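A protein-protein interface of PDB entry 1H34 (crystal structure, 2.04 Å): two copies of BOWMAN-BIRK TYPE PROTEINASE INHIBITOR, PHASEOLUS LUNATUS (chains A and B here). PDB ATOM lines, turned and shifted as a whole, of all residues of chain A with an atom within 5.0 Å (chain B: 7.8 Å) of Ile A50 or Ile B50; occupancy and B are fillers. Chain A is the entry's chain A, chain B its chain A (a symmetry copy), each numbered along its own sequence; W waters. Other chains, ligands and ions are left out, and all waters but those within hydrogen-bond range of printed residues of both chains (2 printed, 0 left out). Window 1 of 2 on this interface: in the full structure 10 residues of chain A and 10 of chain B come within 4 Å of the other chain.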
ATOM      1  N   CYS A  42     -14.090   8.709   6.279  1.00  0.00           N
ATOM      2  CA  CYS A  42     -13.656  10.098   6.414  1.00  0.00           C
ATOM      3  C   CYS A  42     -14.551  10.862   7.378  1.00  0.00           C
ATOM      4  O   CYS A  42     -15.620  10.370   7.742  1.00  0.00           O
ATOM      5  CB  CYS A  42     -13.683  10.756   5.028  1.00  0.00           C
ATOM      6  SG  CYS A  42     -12.463  10.080   3.873  1.00  0.00           S
ATOM      7  N   SER A  48     -15.182  13.983  -0.987  1.00  0.00           N
ATOM      8  CA  SER A  48     -14.473  12.990  -1.779  1.00  0.00           C
ATOM      9  C   SER A  48     -13.623  12.170  -0.797  1.00  0.00           C
ATOM     10  O   SER A  48     -12.549  12.584  -0.374  1.00  0.00           O
ATOM     11  CB  SER A  48     -13.631  13.626  -2.857  1.00  0.00           C
ATOM     12  OG  SER A  48     -12.867  12.679  -3.592  1.00  0.00           O
ATOM     13  N   CYS A  49     -14.120  11.008  -0.414  1.00  0.00           N
ATOM     14  CA  CYS A  49     -13.427  10.099   0.495  1.00  0.00           C
ATOM     15  C   CYS A  49     -12.915   8.873  -0.235  1.00  0.00           C
ATOM     16  O   CYS A  49     -13.734   8.140  -0.800  1.00  0.00           O
ATOM     17  CB  CYS A  49     -14.392   9.627   1.584  1.00  0.00           C
ATOM     18  SG  CYS A  49     -13.532   8.648   2.839  1.00  0.00           S
ATOM     19  N   ILE A  50     -11.611   8.617  -0.296  1.00  0.00           N
ATOM     20  CA  ILE A  50     -11.182   7.403  -1.001  1.00  0.00           C
ATOM     21  C   ILE A  50     -10.567   6.456   0.024  1.00  0.00           C
ATOM     22  O   ILE A  50      -9.973   6.928   1.001  1.00  0.00           O
ATOM     23  CB  ILE A  50     -10.191   7.727  -2.119  1.00  0.00           C
ATOM     24  CG1 ILE A  50      -8.986   8.537  -1.646  1.00  0.00           C
ATOM     25  CG2 ILE A  50     -10.931   8.446  -3.235  1.00  0.00           C
ATOM     26  CD1 ILE A  50      -7.969   8.875  -2.705  1.00  0.00           C
ATOM     27  N   CYS A  51     -10.721   5.153  -0.190  1.00  0.00           N
ATOM     28  CA  CYS A  51     -10.419   4.209   0.893  1.00  0.00           C
ATOM     29  C   CYS A  51      -9.754   2.959   0.349  1.00  0.00           C
ATOM     30  O   CYS A  51      -9.975   2.636  -0.820  1.00  0.00           O
ATOM     31  CB  CYS A  51     -11.682   3.777   1.625  1.00  0.00           C
ATOM     32  SG  CYS A  51     -12.618   4.939   2.573  1.00  0.00           S
ATOM     33  N   THR A  52      -8.968   2.272   1.171  1.00  0.00           N
ATOM     34  CA  THR A  52      -8.392   0.995   0.723  1.00  0.00           C
ATOM     35  C   THR A  52      -9.513  -0.043   0.666  1.00  0.00           C
ATOM     36  O   THR A  52     -10.490   0.085   1.405  1.00  0.00           O
ATOM     37  CB  THR A  52      -7.317   0.464   1.677  1.00  0.00           C
ATOM     38  OG1 THR A  52      -7.838   0.527   3.022  1.00  0.00           O
ATOM     39  CG2 THR A  52      -6.080   1.354   1.660  1.00  0.00           C
ATOM     40  N   GLN A  58      -8.723   1.937   5.222  1.00  0.00           N
ATOM     41  CA  GLN A  58      -7.993   3.173   5.580  1.00  0.00           C
ATOM     42  C   GLN A  58      -8.356   4.247   4.554  1.00  0.00           C
ATOM     43  O   GLN A  58      -8.137   4.025   3.355  1.00  0.00           O
ATOM     44  CB  GLN A  58      -6.495   2.926   5.616  1.00  0.00           C
ATOM     45  CG  GLN A  58      -6.037   1.920   6.684  1.00  0.00           C
ATOM     46  CD  GLN A  58      -4.568   1.559   6.486  1.00  0.00           C
ATOM     47  OE1 GLN A  58      -3.679   2.348   6.807  1.00  0.00           O
ATOM     48  NE2 GLN A  58      -4.305   0.379   5.956  1.00  0.00           N
ATOM     49  N   CYS A  59      -8.887   5.367   5.003  1.00  0.00           N
ATOM     50  CA  CYS A  59      -9.514   6.360   4.152  1.00  0.00           C
ATOM     51  C   CYS A  59      -8.888   7.749   4.215  1.00  0.00           C
ATOM     52  O   CYS A  59      -8.507   8.208   5.303  1.00  0.00           O
ATOM     53  CB  CYS A  59     -10.982   6.492   4.601  1.00  0.00           C
ATOM     54  SG  CYS A  59     -11.912   4.945   4.494  1.00  0.00           S
ATOM     55  N   VAL A  60      -8.829   8.399   3.060  1.00  0.00           N
ATOM     56  CA  VAL A  60      -8.306   9.750   2.888  1.00  0.00           C
ATOM     57  C   VAL A  60      -9.351  10.707   2.318  1.00  0.00           C
ATOM     58  O   VAL A  60      -9.997  10.349   1.324  1.00  0.00           O
ATOM     59  CB  VAL A  60      -7.087   9.737   1.933  1.00  0.00           C
ATOM     60  CG1 VAL A  60      -6.508  11.137   1.795  1.00  0.00           C
ATOM     61  CG2 VAL A  60      -5.994   8.802   2.425  1.00  0.00           C
ATOM     62  N   ASP A  62      -9.976  13.835  -0.024  1.00  0.00           N
ATOM     63  CA  ASP A  62      -9.057  14.799  -0.644  1.00  0.00           C
ATOM     64  C   ASP A  62      -9.745  16.099  -1.036  1.00  0.00           C
ATOM     65  O   ASP A  62      -9.261  16.726  -1.985  1.00  0.00           O
ATOM     66  CB  ASP A  62      -8.360  14.271  -1.886  1.00  0.00           C
ATOM     67  CG  ASP A  62      -9.316  13.332  -2.583  1.00  0.00           C
ATOM     68  OD1 ASP A  62      -8.851  12.177  -2.658  1.00  0.00           O
ATOM     69  OD2 ASP A  62     -10.392  13.866  -2.909  1.00  0.00           O
ATOM     70  N   ASP B  36       1.287  13.011  -0.285  1.00  0.00           N
ATOM     71  CA  ASP B  36       1.035  13.640  -1.587  1.00  0.00           C
ATOM     72  C   ASP B  36      -0.245  13.117  -2.235  1.00  0.00           C
ATOM     73  O   ASP B  36      -0.535  11.925  -2.154  1.00  0.00           O
ATOM     74  CB  ASP B  36       2.169  13.369  -2.577  1.00  0.00           C
ATOM     75  CG  ASP B  36       3.504  13.945  -2.166  1.00  0.00           C
ATOM     76  OD1 ASP B  36       3.570  14.678  -1.160  1.00  0.00           O
ATOM     77  OD2 ASP B  36       4.490  13.631  -2.853  1.00  0.00           O
ATOM     78  N   LEU B  37      -0.985  13.985  -2.889  1.00  0.00           N
ATOM     79  CA  LEU B  37      -2.091  13.611  -3.774  1.00  0.00           C
ATOM     80  C   LEU B  37      -1.547  13.758  -5.187  1.00  0.00           C
ATOM     81  O   LEU B  37      -1.130  14.897  -5.471  1.00  0.00           O
ATOM     82  CB  LEU B  37      -3.232  14.567  -3.556  1.00  0.00           C
ATOM     83  CG  LEU B  37      -4.577  14.200  -3.012  1.00  0.00           C
ATOM     84  CD1 LEU B  37      -5.568  15.334  -3.268  1.00  0.00           C
ATOM     85  CD2 LEU B  37      -5.082  12.919  -3.651  1.00  0.00           C
ATOM     86  N   ARG B  38      -1.515  12.744  -6.032  1.00  0.00           N
ATOM     87  CA  ARG B  38      -0.891  12.851  -7.342  1.00  0.00           C
ATOM     88  C   ARG B  38      -1.866  12.580  -8.489  1.00  0.00           C
ATOM     89  O   ARG B  38      -2.856  11.881  -8.330  1.00  0.00           O
ATOM     90  CB  ARG B  38       0.271  11.871  -7.509  1.00  0.00           C
ATOM     91  CG  ARG B  38       1.457  12.070  -6.584  1.00  0.00           C
ATOM     92  CD  ARG B  38       2.263  10.768  -6.504  1.00  0.00           C
ATOM     93  NE  ARG B  38       2.883  10.504  -7.804  1.00  0.00           N
ATOM     94  CZ  ARG B  38       4.176  10.666  -8.049  1.00  0.00           C
ATOM     95  NH1 ARG B  38       5.013  11.082  -7.110  1.00  0.00           N
ATOM     96  NH2 ARG B  38       4.649  10.408  -9.255  1.00  0.00           N
ATOM     97  N   SER B  41      -1.812   8.463 -11.007  1.00  0.00           N
ATOM     98  CA  SER B  41      -1.261   7.259 -10.377  1.00  0.00           C
ATOM     99  C   SER B  41      -0.243   7.612  -9.299  1.00  0.00           C
ATOM    100  O   SER B  41       0.266   8.734  -9.305  1.00  0.00           O
ATOM    101  CB  SER B  41      -0.588   6.376 -11.439  1.00  0.00           C
ATOM    102  OG  SER B  41       0.696   6.922 -11.730  1.00  0.00           O
ATOM    103  N   CYS B  42       0.033   6.666  -8.412  1.00  0.00           N
ATOM    104  CA  CYS B  42       1.047   6.811  -7.370  1.00  0.00           C
ATOM    105  C   CYS B  42       2.443   6.579  -7.924  1.00  0.00           C
ATOM    106  O   CYS B  42       2.584   6.087  -9.045  1.00  0.00           O
ATOM    107  CB  CYS B  42       0.745   5.805  -6.249  1.00  0.00           C
ATOM    108  SG  CYS B  42      -0.788   6.148  -5.351  1.00  0.00           S
ATOM    109  N   CYS B  46       4.823   2.339  -5.089  1.00  0.00           N
ATOM    110  CA  CYS B  46       3.710   2.314  -4.141  1.00  0.00           C
ATOM    111  C   CYS B  46       2.948   1.003  -4.179  1.00  0.00           C
ATOM    112  O   CYS B  46       2.571   0.506  -5.231  1.00  0.00           O
ATOM    113  CB  CYS B  46       2.698   3.445  -4.406  1.00  0.00           C
ATOM    114  SG  CYS B  46       1.357   3.475  -3.200  1.00  0.00           S
ATOM    115  N   LYS B  47       2.690   0.442  -2.995  1.00  0.00           N
ATOM    116  CA  LYS B  47       2.003  -0.839  -2.983  1.00  0.00           C
ATOM    117  C   LYS B  47       0.509  -0.672  -2.776  1.00  0.00           C
ATOM    118  O   LYS B  47      -0.249  -1.457  -3.308  1.00  0.00           O
ATOM    119  CB  LYS B  47       2.531  -1.733  -1.846  1.00  0.00           C
ATOM    120  CG  LYS B  47       3.950  -2.239  -2.094  1.00  0.00           C
ATOM    121  CD  LYS B  47       4.820  -2.051  -0.862  1.00  0.00           C
ATOM    122  CE  LYS B  47       5.606  -3.309  -0.522  1.00  0.00           C
ATOM    123  NZ  LYS B  47       6.307  -3.174   0.786  1.00  0.00           N
ATOM    124  N   SER B  48       0.108   0.315  -1.973  1.00  0.00           N
ATOM    125  CA  SER B  48      -1.310   0.556  -1.758  1.00  0.00           C
ATOM    126  C   SER B  48      -1.600   1.969  -2.285  1.00  0.00           C
ATOM    127  O   SER B  48      -1.341   2.968  -1.623  1.00  0.00           O
ATOM    128  CB  SER B  48      -1.693   0.406  -0.309  1.00  0.00           C
ATOM    129  OG  SER B  48      -3.059   0.715  -0.063  1.00  0.00           O
ATOM    130  N   CYS B  49      -2.121   2.053  -3.495  1.00  0.00           N
ATOM    131  CA  CYS B  49      -2.476   3.320  -4.130  1.00  0.00           C
ATOM    132  C   CYS B  49      -3.980   3.494  -4.207  1.00  0.00           C
ATOM    133  O   CYS B  49      -4.637   2.663  -4.843  1.00  0.00           O
ATOM    134  CB  CYS B  49      -1.927   3.351  -5.557  1.00  0.00           C
ATOM    135  SG  CYS B  49      -2.181   4.972  -6.320  1.00  0.00           S
ATOM    136  N   ILE B  50      -4.579   4.497  -3.572  1.00  0.00           N
ATOM    137  CA  ILE B  50      -6.035   4.623  -3.704  1.00  0.00           C
ATOM    138  C   ILE B  50      -6.330   5.909  -4.469  1.00  0.00           C
ATOM    139  O   ILE B  50      -5.567   6.874  -4.341  1.00  0.00           O
ATOM    140  CB  ILE B  50      -6.722   4.622  -2.338  1.00  0.00           C
ATOM    141  CG1 ILE B  50      -6.169   5.674  -1.380  1.00  0.00           C
ATOM    142  CG2 ILE B  50      -6.618   3.228  -1.739  1.00  0.00           C
ATOM    143  CD1 ILE B  50      -6.818   5.727  -0.021  1.00  0.00           C
ATOM    144  N   CYS B  51      -7.403   5.911  -5.253  1.00  0.00           N
ATOM    145  CA  CYS B  51      -7.574   6.994  -6.229  1.00  0.00           C
ATOM    146  C   CYS B  51      -9.031   7.405  -6.329  1.00  0.00           C
ATOM    147  O   CYS B  51      -9.897   6.575  -6.046  1.00  0.00           O
ATOM    148  CB  CYS B  51      -7.118   6.571  -7.618  1.00  0.00           C
ATOM    149  SG  CYS B  51      -5.416   6.221  -7.944  1.00  0.00           S
ATOM    150  N   THR B  52      -9.295   8.646  -6.727  1.00  0.00           N
ATOM    151  CA  THR B  52     -10.691   9.053  -6.946  1.00  0.00           C
ATOM    152  C   THR B  52     -11.197   8.366  -8.214  1.00  0.00           C
ATOM    153  O   THR B  52     -10.392   8.055  -9.094  1.00  0.00           O
ATOM    154  CB  THR B  52     -10.841  10.565  -7.147  1.00  0.00           C
ATOM    155  OG1 THR B  52      -9.860  10.990  -8.119  1.00  0.00           O
ATOM    156  CG2 THR B  52     -10.522  11.324  -5.864  1.00  0.00           C
ATOM    157  N   LEU B  53     -12.489   8.148  -8.314  1.00  0.00           N
ATOM    158  CA  LEU B  53     -13.085   7.577  -9.519  1.00  0.00           C
ATOM    159  C   LEU B  53     -13.397   8.699 -10.505  1.00  0.00           C
ATOM    160  O   LEU B  53     -14.553   9.000 -10.790  1.00  0.00           O
ATOM    161  CB  LEU B  53     -14.386   6.854  -9.203  1.00  0.00           C
ATOM    162  CG  LEU B  53     -14.376   5.517  -8.474  1.00  0.00           C
ATOM    163  CD1 LEU B  53     -13.185   4.669  -8.902  1.00  0.00           C
ATOM    164  CD2 LEU B  53     -14.394   5.749  -6.974  1.00  0.00           C
ATOM    165  N   ALA B  57      -7.362  11.090 -12.476  1.00  0.00           N
ATOM    166  CA  ALA B  57      -7.579  10.505 -11.156  1.00  0.00           C
ATOM    167  C   ALA B  57      -6.735  11.250 -10.131  1.00  0.00           C
ATOM    168  O   ALA B  57      -5.608  11.653 -10.435  1.00  0.00           O
ATOM    169  CB  ALA B  57      -7.228   9.012 -11.144  1.00  0.00           C
ATOM    170  N   GLN B  58      -7.252  11.406  -8.916  1.00  0.00           N
ATOM    171  CA  GLN B  58      -6.308  11.943  -7.911  1.00  0.00           C
ATOM    172  C   GLN B  58      -5.987  10.824  -6.920  1.00  0.00           C
ATOM    173  O   GLN B  58      -6.919  10.291  -6.301  1.00  0.00           O
ATOM    174  CB  GLN B  58      -6.897  13.153  -7.208  1.00  0.00           C
ATOM    175  CG  GLN B  58      -7.168  14.358  -8.124  1.00  0.00           C
ATOM    176  CD  GLN B  58      -7.972  15.423  -7.384  1.00  0.00           C
ATOM    177  OE1 GLN B  58      -7.436  16.146  -6.544  1.00  0.00           O
ATOM    178  NE2 GLN B  58      -9.255  15.524  -7.685  1.00  0.00           N
ATOM    179  N   CYS B  59      -4.723  10.481  -6.772  1.00  0.00           N
ATOM    180  CA  CYS B  59      -4.287   9.285  -6.078  1.00  0.00           C
ATOM    181  C   CYS B  59      -3.371   9.532  -4.884  1.00  0.00           C
ATOM    182  O   CYS B  59      -2.493  10.406  -4.948  1.00  0.00           O
ATOM    183  CB  CYS B  59      -3.511   8.421  -7.089  1.00  0.00           C
ATOM    184  SG  CYS B  59      -4.489   7.946  -8.534  1.00  0.00           S
ATOM    185  N   VAL B  60      -3.568   8.736  -3.841  1.00  0.00           N
ATOM    186  CA  VAL B  60      -2.788   8.765  -2.609  1.00  0.00           C
ATOM    187  C   VAL B  60      -2.098   7.432  -2.328  1.00  0.00           C
ATOM    188  O   VAL B  60      -2.769   6.394  -2.406  1.00  0.00           O
ATOM    189  CB  VAL B  60      -3.700   9.104  -1.405  1.00  0.00           C
ATOM    190  CG1 VAL B  60      -2.878   9.188  -0.127  1.00  0.00           C
ATOM    191  CG2 VAL B  60      -4.433  10.421  -1.602  1.00  0.00           C
ATOM    192  N   CYS B  61      -0.809   7.415  -1.994  1.00  0.00           N
ATOM    193  CA  CYS B  61      -0.157   6.171  -1.553  1.00  0.00           C
ATOM    194  C   CYS B  61      -0.341   6.005  -0.064  1.00  0.00           C
ATOM    195  O   CYS B  61       0.046   6.898   0.720  1.00  0.00           O
ATOM    196  CB  CYS B  61       1.340   6.168  -1.855  1.00  0.00           C
ATOM    197  SG  CYS B  61       2.184   4.572  -1.624  1.00  0.00           S
ATOM    198  N   ASP B  62      -0.910   4.900   0.472  1.00  0.00           N
ATOM    199  CA  ASP B  62      -0.798   5.030   1.931  1.00  0.00           C
ATOM    200  C   ASP B  62       0.156   4.011   2.540  1.00  0.00           C
ATOM    201  O   ASP B  62      -0.058   3.671   3.708  1.00  0.00           O
ATOM    202  CB  ASP B  62      -2.123   4.893   2.663  1.00  0.00           C
ATOM    203  CG  ASP B  62      -2.975   3.915   1.888  1.00  0.00           C
ATOM    204  OD1 ASP B  62      -4.028   4.446   1.483  1.00  0.00           O
ATOM    205  OD2 ASP B  62      -2.455   2.791   1.762  1.00  0.00           O
HETATM  206  O   HOH W   1      -8.884  17.529  -4.775  1.00  0.00           O
HETATM  207  O   HOH W   2      -1.184   2.075   5.888  1.00  0.00           O
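Of the 10 printed residues of chain A, 5 touch a printed residue of chain B. Hydrophobic or aromatic side chains of chain A that line the printed part of chain B: Ile A50. Hydrophobic or aromatic side chains of chain B within 4 Å of the printed part of chain A: Leu B37 and Ile B50. Among the printed residues, 10 pairs touch across the chains. Among the printed residues, no Asp or Glu carboxylate lies within 4 Å of a Lys or Arg side-chain nitrogen of the other chain.
Among the printed residues, pairs that only touch across the chains: Ser A48 with Thr B52, Ile A50 with Ile B50, Ile A50 with Cys B51, Ile A50 with Thr B52, Cys A51 with Ile B50, Thr A52 with Ser B48, Thr A52 with Ile B50, Thr A52 with Asp B62, Asp A62 with Leu B37 and Asp A62 with Thr B52.
Of the printed residues of chain B, Ser A48 touches Thr B52 (3.5 Å). No residue of chain B comes within 4 Å of Cys A49. Printed residues of chain B within 4 Å of Ile A50: Ile B50, Cys B51 and Thr B52. Cys A51 touches just one residue of chain B: Ile B50 (3.5 Å). Of the printed residues of chain B, Thr A52 touches Ser B48 (3.5 Å), Ile B50 (3.8 Å) and Asp B62 (3.7 Å). Printed residues of chain A within 4 Å of Leu B37: Asp A62 (3.3 Å). Cys B46 touches none of the printed residues of chain A. Of the printed residues of chain A, Ser B48 touches Thr A52 (3.5 Å). Printed residues of chain A within 4 Å of Ile B50: Ile A50 (3.5 Å), Cys A51 (3.5 Å) and Thr A52 (3.8 Å). Printed residues of chain A within 4 Å of Cys B51: Ile A50. Ala B57 touches none of the printed residues of chain A. The nearest printed residue of chain B that does not touch Ile A50 is Gln B58 (4.005 Å). The nearest printed residue of chain B that does not touch Ser A48 is Gln B58 (6.2 Å).
OD2 of Asp A62 sits at hydrogen-bond distance from OG of Ser A48 (2.8 Å). The backbone carbonyl oxygen (O) of Ile A50 lies within hydrogen-bond range of the backbone NH (N) of Val A60 (2.8 Å). The backbone NH (N) of Ser B48 lies close to the side-chain sulfur (SG) of Cys B46 (3.6 Å). The backbone NH of Val B60 sits at hydrogen-bond distance from the backbone carbonyl oxygen of Ile B50, at 2.8 Å. The side-chain sulfur (SG) of Cys A49 is disulfide-bonded to the side-chain sulfur (SG) of Cys A42 (2.1 Å). The side-chain sulfur (SG) of Cys B42 forms a disulfide with the side-chain sulfur (SG) of Cys B49 (2.1 Å).
Water W1 lies within hydrogen-bond range of the side-chain amide oxygen of Gln B58 and the backbone carbonyl oxygen of Asp A62. Water W2 bridges OE1 of Gln A58 (2.7 Å) and O of Asp B62 (2.9 Å).
Ser A48 touches Thr B52, and with the chains exchanged Thr A52 touches Ser B48. Ile B50 touches its own counterpart, Ile A50. Ile A50 touches Thr B52, and with the chains exchanged Thr A52 touches Ile B50. Thr A52 touches Asp B62, and with the chains exchanged Asp A62 touches Thr B52. Positions printed for both chains: 42, 48, 49, 50, 51, 52, 58, 59, 60 and 62. Of the 10 pairs that touch across the chains among the printed residues, 9 have their exchanged pair printed and touching as well.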
